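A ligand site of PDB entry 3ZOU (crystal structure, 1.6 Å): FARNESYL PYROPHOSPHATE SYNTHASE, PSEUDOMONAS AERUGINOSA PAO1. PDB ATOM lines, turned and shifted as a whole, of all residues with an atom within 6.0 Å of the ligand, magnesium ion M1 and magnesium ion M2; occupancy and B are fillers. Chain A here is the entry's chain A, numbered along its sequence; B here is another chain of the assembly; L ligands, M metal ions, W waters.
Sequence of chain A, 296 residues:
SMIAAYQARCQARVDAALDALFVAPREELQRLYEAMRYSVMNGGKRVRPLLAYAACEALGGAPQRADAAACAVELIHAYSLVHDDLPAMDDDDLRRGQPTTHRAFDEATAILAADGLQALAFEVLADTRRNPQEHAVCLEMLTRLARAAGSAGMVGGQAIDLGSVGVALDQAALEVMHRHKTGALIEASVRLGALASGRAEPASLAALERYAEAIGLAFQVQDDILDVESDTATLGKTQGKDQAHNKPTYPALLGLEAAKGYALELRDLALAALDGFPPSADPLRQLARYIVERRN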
ATOM      1  N   ARG A  48     -11.002 -28.250  12.459  1.00  0.00           N
ATOM      2  CA  ARG A  48     -11.116 -29.255  11.445  1.00  0.00           C
ATOM      3  C   ARG A  48      -9.787 -29.901  11.043  1.00  0.00           C
ATOM      4  O   ARG A  48      -9.690 -31.142  11.079  1.00  0.00           O
ATOM      5  CB  ARG A  48     -11.901 -28.662  10.265  1.00  0.00           C
ATOM      6  CG  ARG A  48     -13.378 -28.440  10.597  1.00  0.00           C
ATOM      7  CD  ARG A  48     -14.023 -27.459   9.664  1.00  0.00           C
ATOM      8  NE  ARG A  48     -15.364 -27.119  10.167  1.00  0.00           N
ATOM      9  CZ  ARG A  48     -15.560 -26.247  11.140  1.00  0.00           C
ATOM     10  NH1 ARG A  48     -14.553 -25.581  11.713  1.00  0.00           N
ATOM     11  NH2 ARG A  48     -16.781 -26.021  11.576  1.00  0.00           N
ATOM     12  N   HIS A  77     -13.737 -24.843   4.855  1.00  0.00           N
ATOM     13  CA  HIS A  77     -14.254 -24.077   5.952  1.00  0.00           C
ATOM     14  C   HIS A  77     -14.091 -22.536   5.732  1.00  0.00           C
ATOM     15  O   HIS A  77     -15.053 -21.783   5.788  1.00  0.00           O
ATOM     16  CB  HIS A  77     -13.595 -24.506   7.262  1.00  0.00           C
ATOM     17  CG  HIS A  77     -14.107 -23.782   8.453  1.00  0.00           C
ATOM     18  ND1 HIS A  77     -15.430 -23.705   8.801  1.00  0.00           N
ATOM     19  CD2 HIS A  77     -13.441 -23.033   9.358  1.00  0.00           C
ATOM     20  CE1 HIS A  77     -15.544 -22.979   9.890  1.00  0.00           C
ATOM     21  NE2 HIS A  77     -14.353 -22.556  10.231  1.00  0.00           N
ATOM     22  N   TYR A  79     -13.532 -20.911   2.910  1.00  0.00           N
ATOM     23  CA  TYR A  79     -14.290 -20.361   1.737  1.00  0.00           C
ATOM     24  C   TYR A  79     -15.753 -20.189   2.202  1.00  0.00           C
ATOM     25  O   TYR A  79     -16.398 -19.150   1.885  1.00  0.00           O
ATOM     26  CB  TYR A  79     -14.180 -21.193   0.480  1.00  0.00           C
ATOM     27  CG  TYR A  79     -15.472 -21.904   0.042  1.00  0.00           C
ATOM     28  CD1 TYR A  79     -16.500 -21.189  -0.503  1.00  0.00           C
ATOM     29  CD2 TYR A  79     -15.645 -23.261   0.160  1.00  0.00           C
ATOM     30  CE1 TYR A  79     -17.681 -21.806  -0.882  1.00  0.00           C
ATOM     31  CE2 TYR A  79     -16.832 -23.885  -0.196  1.00  0.00           C
ATOM     32  CZ  TYR A  79     -17.839 -23.166  -0.730  1.00  0.00           C
ATOM     33  OH  TYR A  79     -19.006 -23.788  -1.040  1.00  0.00           O
ATOM     34  N   SER A  80     -16.276 -21.129   2.999  1.00  0.00           N
ATOM     35  CA  SER A  80     -17.692 -21.056   3.401  1.00  0.00           C
ATOM     36  C   SER A  80     -17.972 -19.868   4.263  1.00  0.00           C
ATOM     37  O   SER A  80     -19.008 -19.222   4.083  1.00  0.00           O
ATOM     38  CB  SER A  80     -18.099 -22.367   4.087  1.00  0.00           C
ATOM     39  OG  SER A  80     -17.645 -22.401   5.425  1.00  0.00           O
ATOM     40  N   LEU A  81     -17.011 -19.437   5.081  1.00  0.00           N
ATOM     41  CA  LEU A  81     -17.217 -18.267   5.975  1.00  0.00           C
ATOM     42  C   LEU A  81     -17.216 -16.972   5.164  1.00  0.00           C
ATOM     43  O   LEU A  81     -17.985 -16.082   5.438  1.00  0.00           O
ATOM     44  CB  LEU A  81     -16.143 -18.275   7.075  1.00  0.00           C
ATOM     45  CG  LEU A  81     -16.211 -19.480   8.048  1.00  0.00           C
ATOM     46  CD1 LEU A  81     -15.102 -19.250   9.096  1.00  0.00           C
ATOM     47  CD2 LEU A  81     -17.610 -19.698   8.599  1.00  0.00           C
ATOM     48  N   HIS A  83     -18.214 -16.607   2.050  1.00  0.00           N
ATOM     49  CA  HIS A  83     -19.528 -16.470   1.393  1.00  0.00           C
ATOM     50  C   HIS A  83     -20.622 -16.176   2.419  1.00  0.00           C
ATOM     51  O   HIS A  83     -21.503 -15.416   2.113  1.00  0.00           O
ATOM     52  CB  HIS A  83     -19.834 -17.651   0.493  1.00  0.00           C
ATOM     53  CG  HIS A  83     -19.086 -17.647  -0.808  1.00  0.00           C
ATOM     54  ND1 HIS A  83     -19.288 -18.579  -1.795  1.00  0.00           N
ATOM     55  CD2 HIS A  83     -18.150 -16.790  -1.293  1.00  0.00           C
ATOM     56  CE1 HIS A  83     -18.503 -18.331  -2.821  1.00  0.00           C
ATOM     57  NE2 HIS A  83     -17.786 -17.252  -2.540  1.00  0.00           N
ATOM     58  N   ASP A  84     -20.578 -16.828   3.569  1.00  0.00           N
ATOM     59  CA  ASP A  84     -21.581 -16.632   4.642  1.00  0.00           C
ATOM     60  C   ASP A  84     -21.591 -15.132   5.066  1.00  0.00           C
ATOM     61  O   ASP A  84     -22.649 -14.613   5.418  1.00  0.00           O
ATOM     62  CB  ASP A  84     -21.256 -17.485   5.828  1.00  0.00           C
ATOM     63  CG  ASP A  84     -22.249 -17.361   6.968  1.00  0.00           C
ATOM     64  OD1 ASP A  84     -23.426 -17.827   6.843  1.00  0.00           O
ATOM     65  OD2 ASP A  84     -21.884 -16.764   7.991  1.00  0.00           O
ATOM     66  N   ASP A  85     -20.463 -14.462   5.045  1.00  0.00           N
ATOM     67  CA  ASP A  85     -20.369 -13.105   5.539  1.00  0.00           C
ATOM     68  C   ASP A  85     -20.933 -12.090   4.532  1.00  0.00           C
ATOM     69  O   ASP A  85     -21.171 -10.947   4.861  1.00  0.00           O
ATOM     70  CB  ASP A  85     -18.914 -12.749   5.808  1.00  0.00           C
ATOM     71  CG  ASP A  85     -18.339 -13.368   7.065  1.00  0.00           C
ATOM     72  OD1 ASP A  85     -19.073 -13.683   8.008  1.00  0.00           O
ATOM     73  OD2 ASP A  85     -17.113 -13.479   7.106  1.00  0.00           O
ATOM     74  N   MET A  89     -26.022 -12.853   2.286  1.00  0.00           N
ATOM     75  CA  MET A  89     -26.152 -13.901   3.271  1.00  0.00           C
ATOM     76  C   MET A  89     -26.219 -13.244   4.625  1.00  0.00           C
ATOM     77  O   MET A  89     -27.249 -12.664   4.943  1.00  0.00           O
ATOM     78  CB  MET A  89     -24.948 -14.887   3.192  1.00  0.00           C
ATOM     79  CG  MET A  89     -24.827 -15.472   1.810  1.00  0.00           C
ATOM     80  SD  MET A  89     -25.223 -17.227   1.758  1.00  0.00           S
ATOM     81  CE  MET A  89     -24.067 -17.480   0.420  1.00  0.00           C
ATOM     82  N   ASP A  90     -25.166 -13.332   5.450  1.00  0.00           N
ATOM     83  CA  ASP A  90     -25.296 -12.734   6.816  1.00  0.00           C
ATOM     84  C   ASP A  90     -24.946 -11.240   6.900  1.00  0.00           C
ATOM     85  O   ASP A  90     -25.206 -10.601   7.931  1.00  0.00           O
ATOM     86  CB  ASP A  90     -24.515 -13.541   7.828  1.00  0.00           C
ATOM     87  CG  ASP A  90     -25.163 -14.849   8.102  1.00  0.00           C
ATOM     88  OD1 ASP A  90     -26.374 -15.054   7.738  1.00  0.00           O
ATOM     89  OD2 ASP A  90     -24.454 -15.691   8.659  1.00  0.00           O
ATOM     90  N   ASP A  92     -22.112  -9.517   7.303  1.00  0.00           N
ATOM     91  CA  ASP A  92     -21.292  -9.186   8.427  1.00  0.00           C
ATOM     92  C   ASP A  92     -20.097  -8.341   8.051  1.00  0.00           C
ATOM     93  O   ASP A  92     -19.354  -8.672   7.128  1.00  0.00           O
ATOM     94  CB  ASP A  92     -20.878 -10.451   9.167  1.00  0.00           C
ATOM     95  CG  ASP A  92     -21.913 -10.858  10.235  1.00  0.00           C
ATOM     96  OD1 ASP A  92     -22.307  -9.974  10.988  1.00  0.00           O
ATOM     97  OD2 ASP A  92     -22.357 -11.997  10.237  1.00  0.00           O
ATOM     98  N   ARG A  95     -15.600 -10.411  11.420  1.00  0.00           N
ATOM     99  CA  ARG A  95     -15.503 -11.795  11.831  1.00  0.00           C
ATOM    100  C   ARG A  95     -14.421 -11.864  12.895  1.00  0.00           C
ATOM    101  O   ARG A  95     -13.257 -11.498  12.661  1.00  0.00           O
ATOM    102  CB  ARG A  95     -15.177 -12.694  10.631  1.00  0.00           C
ATOM    103  CG  ARG A  95     -15.060 -14.170  11.101  1.00  0.00           C
ATOM    104  CD  ARG A  95     -15.104 -15.128   9.922  1.00  0.00           C
ATOM    105  NE  ARG A  95     -16.458 -15.289   9.415  1.00  0.00           N
ATOM    106  CZ  ARG A  95     -17.453 -16.010   9.950  1.00  0.00           C
ATOM    107  NH1 ARG A  95     -17.282 -16.709  11.110  1.00  0.00           N
ATOM    108  NH2 ARG A  95     -18.634 -16.074   9.356  1.00  0.00           N
ATOM    109  N   ALA A 149     -18.869 -31.148   1.172  1.00  0.00           N
ATOM    110  CA  ALA A 149     -18.781 -29.685   0.969  1.00  0.00           C
ATOM    111  C   ALA A 149     -19.976 -29.204   0.136  1.00  0.00           C
ATOM    112  O   ALA A 149     -20.282 -27.992   0.212  1.00  0.00           O
ATOM    113  CB  ALA A 149     -17.540 -29.300   0.271  1.00  0.00           C
ATOM    114  N   MET A 154     -22.551 -29.354   3.335  1.00  0.00           N
ATOM    115  CA  MET A 154     -22.387 -28.047   3.862  1.00  0.00           C
ATOM    116  C   MET A 154     -23.248 -26.963   3.149  1.00  0.00           C
ATOM    117  O   MET A 154     -23.920 -26.197   3.802  1.00  0.00           O
ATOM    118  CB  MET A 154     -20.916 -27.669   3.838  1.00  0.00           C
ATOM    119  CG  MET A 154     -20.550 -26.311   4.395  1.00  0.00           C
ATOM    120  SD  MET A 154     -18.835 -25.857   4.163  1.00  0.00           S
ATOM    121  CE  MET A 154     -18.895 -25.413   2.428  1.00  0.00           C
ATOM    122  N   VAL A 155     -23.167 -26.927   1.832  1.00  0.00           N
ATOM    123  CA  VAL A 155     -23.924 -25.947   1.082  1.00  0.00           C
ATOM    124  C   VAL A 155     -25.396 -26.182   1.249  1.00  0.00           C
ATOM    125  O   VAL A 155     -26.156 -25.261   1.474  1.00  0.00           O
ATOM    126  CB  VAL A 155     -23.497 -25.957  -0.410  1.00  0.00           C
ATOM    127  CG1 VAL A 155     -24.533 -25.209  -1.283  1.00  0.00           C
ATOM    128  CG2 VAL A 155     -22.156 -25.349  -0.576  1.00  0.00           C
ATOM    129  N   GLY A 156     -25.788 -27.451   1.254  1.00  0.00           N
ATOM    130  CA  GLY A 156     -27.174 -27.848   1.600  1.00  0.00           C
ATOM    131  C   GLY A 156     -27.581 -27.316   2.960  1.00  0.00           C
ATOM    132  O   GLY A 156     -28.654 -26.757   3.114  1.00  0.00           O
ATOM    133  N   GLN A 158     -26.416 -24.732   4.567  1.00  0.00           N
ATOM    134  CA  GLN A 158     -26.538 -23.288   4.465  1.00  0.00           C
ATOM    135  C   GLN A 158     -27.903 -22.965   3.864  1.00  0.00           C
ATOM    136  O   GLN A 158     -28.558 -22.063   4.380  1.00  0.00           O
ATOM    137  CB  GLN A 158     -25.405 -22.673   3.689  1.00  0.00           C
ATOM    138  CG  GLN A 158     -25.457 -21.158   3.652  1.00  0.00           C
ATOM    139  CD  GLN A 158     -25.081 -20.397   4.930  1.00  0.00           C
ATOM    140  OE1 GLN A 158     -25.079 -21.063   6.091  1.00  0.00           O
ATOM    141  NE2 GLN A 158     -24.780 -19.152   4.850  1.00  0.00           N
ATOM    142  N   ASP A 161     -30.565 -23.618   6.484  1.00  0.00           N
ATOM    143  CA  ASP A 161     -30.528 -22.507   7.458  1.00  0.00           C
ATOM    144  C   ASP A 161     -31.256 -21.284   6.878  1.00  0.00           C
ATOM    145  O   ASP A 161     -32.229 -20.741   7.486  1.00  0.00           O
ATOM    146  CB  ASP A 161     -29.123 -22.196   7.864  1.00  0.00           C
ATOM    147  CG  ASP A 161     -28.999 -21.300   9.093  1.00  0.00           C
ATOM    148  OD1 ASP A 161     -29.952 -21.246   9.893  1.00  0.00           O
ATOM    149  OD2 ASP A 161     -27.889 -20.809   9.332  1.00  0.00           O
ATOM    150  N   LEU A 162     -30.902 -20.913   5.671  1.00  0.00           N
ATOM    151  CA  LEU A 162     -31.540 -19.786   5.044  1.00  0.00           C
ATOM    152  C   LEU A 162     -33.012 -20.001   4.824  1.00  0.00           C
ATOM    153  O   LEU A 162     -33.767 -19.067   4.975  1.00  0.00           O
ATOM    154  CB  LEU A 162     -30.846 -19.464   3.725  1.00  0.00           C
ATOM    155  CG  LEU A 162     -29.501 -18.787   4.043  1.00  0.00           C
ATOM    156  CD1 LEU A 162     -28.800 -18.644   2.700  1.00  0.00           C
ATOM    157  CD2 LEU A 162     -29.577 -17.423   4.733  1.00  0.00           C
ATOM    158  N   LYS A 181     -25.032 -28.359   7.946  1.00  0.00           N
ATOM    159  CA  LYS A 181     -24.319 -27.103   7.845  1.00  0.00           C
ATOM    160  C   LYS A 181     -22.936 -27.177   8.426  1.00  0.00           C
ATOM    161  O   LYS A 181     -21.984 -26.562   7.898  1.00  0.00           O
ATOM    162  CB  LYS A 181     -25.092 -25.979   8.521  1.00  0.00           C
ATOM    163  CG  LYS A 181     -24.496 -24.602   8.239  1.00  0.00           C
ATOM    164  CD  LYS A 181     -25.363 -23.488   8.701  1.00  0.00           C
ATOM    165  CE  LYS A 181     -25.282 -23.378  10.192  1.00  0.00           C
ATOM    166  NZ  LYS A 181     -25.746 -22.007  10.613  1.00  0.00           N
ATOM    167  N   THR A 182     -22.834 -27.837   9.562  1.00  0.00           N
ATOM    168  CA  THR A 182     -21.509 -28.068  10.174  1.00  0.00           C
ATOM    169  C   THR A 182     -21.132 -29.547  10.318  1.00  0.00           C
ATOM    170  O   THR A 182     -19.931 -29.875  10.238  1.00  0.00           O
ATOM    171  CB  THR A 182     -21.366 -27.320  11.497  1.00  0.00           C
ATOM    172  OG1 THR A 182     -22.454 -27.673  12.317  1.00  0.00           O
ATOM    173  CG2 THR A 182     -21.330 -25.842  11.303  1.00  0.00           C
ATOM    174  N   LEU B 112     -25.093 -20.012  -3.438  1.00  0.00           N
ATOM    175  CA  LEU B 112     -25.033 -21.368  -2.913  1.00  0.00           C
ATOM    176  C   LEU B 112     -25.141 -22.431  -3.997  1.00  0.00           C
ATOM    177  O   LEU B 112     -24.375 -23.390  -4.011  1.00  0.00           O
ATOM    178  CB  LEU B 112     -26.079 -21.571  -1.835  1.00  0.00           C
ATOM    179  CG  LEU B 112     -25.871 -20.781  -0.596  1.00  0.00           C
ATOM    180  CD1 LEU B 112     -27.064 -20.906   0.331  1.00  0.00           C
ATOM    181  CD2 LEU B 112     -24.587 -21.131   0.161  1.00  0.00           C
ATOM    182  N   ASP B 115     -21.892 -22.591  -5.729  1.00  0.00           N
ATOM    183  CA  ASP B 115     -20.859 -23.199  -4.865  1.00  0.00           C
ATOM    184  C   ASP B 115     -21.047 -24.737  -4.894  1.00  0.00           C
ATOM    185  O   ASP B 115     -20.022 -25.479  -4.938  1.00  0.00           O
ATOM    186  CB  ASP B 115     -21.012 -22.704  -3.445  1.00  0.00           C
ATOM    187  CG  ASP B 115     -20.496 -21.326  -3.209  1.00  0.00           C
ATOM    188  OD1 ASP B 115     -19.744 -20.793  -4.001  1.00  0.00           O
ATOM    189  OD2 ASP B 115     -20.875 -20.701  -2.147  1.00  0.00           O
HETATM  190  C1  LIG L   1     -21.510 -20.063   9.432  1.00  0.00           C
HETATM  191  O1  LIG L   1     -22.754 -20.194  10.162  1.00  0.00           O
HETATM  192  C2  LIG L   1     -21.635 -20.725   8.105  1.00  0.00           C
HETATM  193  C3  LIG L   1     -21.341 -22.029   7.904  1.00  0.00           C
HETATM  194  C4  LIG L   1     -20.724 -22.767   9.014  1.00  0.00           C
HETATM  195  C5  LIG L   1     -21.441 -22.664   6.580  1.00  0.00           C
HETATM  196  C6  LIG L   1     -21.522 -21.584   5.487  1.00  0.00           C
HETATM  197  C7  LIG L   1     -21.785 -22.279   4.225  1.00  0.00           C
HETATM  198  C8  LIG L   1     -21.770 -21.761   3.007  1.00  0.00           C
HETATM  199  C9  LIG L   1     -21.439 -20.327   2.580  1.00  0.00           C
HETATM  200  C10 LIG L   1     -22.142 -22.872   2.063  1.00  0.00           C
HETATM  201  P1  LIG L   1     -23.330 -18.927  10.959  1.00  0.00           P
HETATM  202  O2  LIG L   1     -23.666 -17.801   9.946  1.00  0.00           O
HETATM  203  O3  LIG L   1     -24.517 -19.459  11.739  1.00  0.00           O
HETATM  204  O4  LIG L   1     -22.118 -18.669  11.973  1.00  0.00           O
HETATM  205  P2  LIG L   1     -21.157 -17.380  12.125  1.00  0.00           P
HETATM  206  O5  LIG L   1     -21.517 -16.475  10.951  1.00  0.00           O
HETATM  207  O6  LIG L   1     -21.514 -16.736  13.455  1.00  0.00           O
HETATM  208  O7  LIG L   1     -19.792 -18.050  12.057  1.00  0.00           O
HETATM  209 MG    MG M   1     -24.965 -17.741   8.410  1.00  0.00          MG
HETATM  210 MG    MG M   2     -22.784 -15.962   9.694  1.00  0.00          MG
HETATM  211  O   HOH W   1     -20.222 -14.337  12.125  1.00  0.00           O
HETATM  212  O   HOH W   2     -26.664 -17.607   9.690  1.00  0.00           O
HETATM  213  O   HOH W   3     -21.781 -14.213   9.196  1.00  0.00           O
HETATM  214  O   HOH W   4     -26.380 -17.391   6.849  1.00  0.00           O
HETATM  215  O   HOH W   5     -18.741 -20.309  12.261  1.00  0.00           O
HETATM  216  O   HOH W   6     -25.314 -19.939   8.334  1.00  0.00           O
HETATM  217  O   HOH W   7     -23.792 -14.945  11.171  1.00  0.00           O
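The guanidinium group (NH1) of Arg 95 is in salt-bridge range of an oxygen (O7) of the ligand (3.0 Å). The side-chain amino group of Lys 181 is in salt-bridge range of an oxygen (O3) of the ligand (3.0 Å).
The side-chain carboxylate (OD2) of Asp 84 sits close to the guanidinium group (NH2) of Arg 95. OD1 of Asp 84 lies close to NE2 of Gln 158 (2.7 Å). The guanidinium group of Arg 95 is in salt-bridge range of the side-chain carboxylate of Asp 85, at 2.8 Å. The side-chain amino group (NZ) of Lys 181 is in salt-bridge range of the side-chain carboxylate (OD2) of Asp 161, at 2.8 Å. OG of Ser 80 lies within hydrogen-bond range of O of His 77 (2.7 Å). The backbone carbonyl oxygen (O) of Ala 149 sits close to the backbone NH (N) of Val 155 (3.5 Å). The side-chain amide nitrogen (NE2) of Gln 158 is in hydrogen-bond range of the side-chain sulfur (SD) of Met 89 (3.7 Å). OD2 of Asp 115 of chain B sits at hydrogen-bond distance from ND1 of His 83, at 2.7 Å.
Ser 80 touches the ligand. His 83 touches the ligand. CG2 of Val 155 touches C10 of the ligand, 3.6 Å away. Gln 158 touches the ligand (OE1 to C6, 3.6 Å). Thr 182 touches the ligand. Leu 112 of chain B touches the ligand. Hydrophobic or aromatic side chains within 4 Å of the ligand: His 83, Val 155 and Leu 112 of chain B. Within 4 Å of the ligand: Ser 80, His 83, Asp 84, Asp 90, Arg 95, Val 155, Gln 158, Lys 181, Thr 182 and Leu 112 of chain B.
Merely in contact with magnesium ion M1: Gln 158 (3.8 Å).
Magnesium ion M1 is bound by O2 of the ligand (2.0 Å), OD2 of Asp 90 (2.1 Å), water W2 (2.1 Å), water W4 (2.1 Å), OD1 of Asp 84 (2.2 Å) and water W6 (2.2 Å). Magnesium ion M1 has six donor atoms within binding distance.
Magnesium ion M2 is bound by an oxygen (O5) of the ligand (1.9 Å), the side-chain carboxylate of Asp 90 (2.0 Å), an oxygen (O2) of the ligand (2.1 Å), water W7 (2.1 Å), water W3 (2.1 Å) and the side-chain carboxylate of Asp 84 (2.1 Å). Magnesium ion M2 has six donor atoms within binding distance.
Water W2 lies within hydrogen-bond range of OD1 of Asp 90, OD2 of Asp 161 and O3 of the ligand. Water W4 bridges the side-chain carboxylate of Asp 90 (2.5 Å) and the side-chain amide nitrogen of Gln 158 (3.1 Å). Water W3 lies within hydrogen-bond range of OD2 of Asp 92 (2.5 Å) and OD1 of Asp 85 (3.0 Å).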
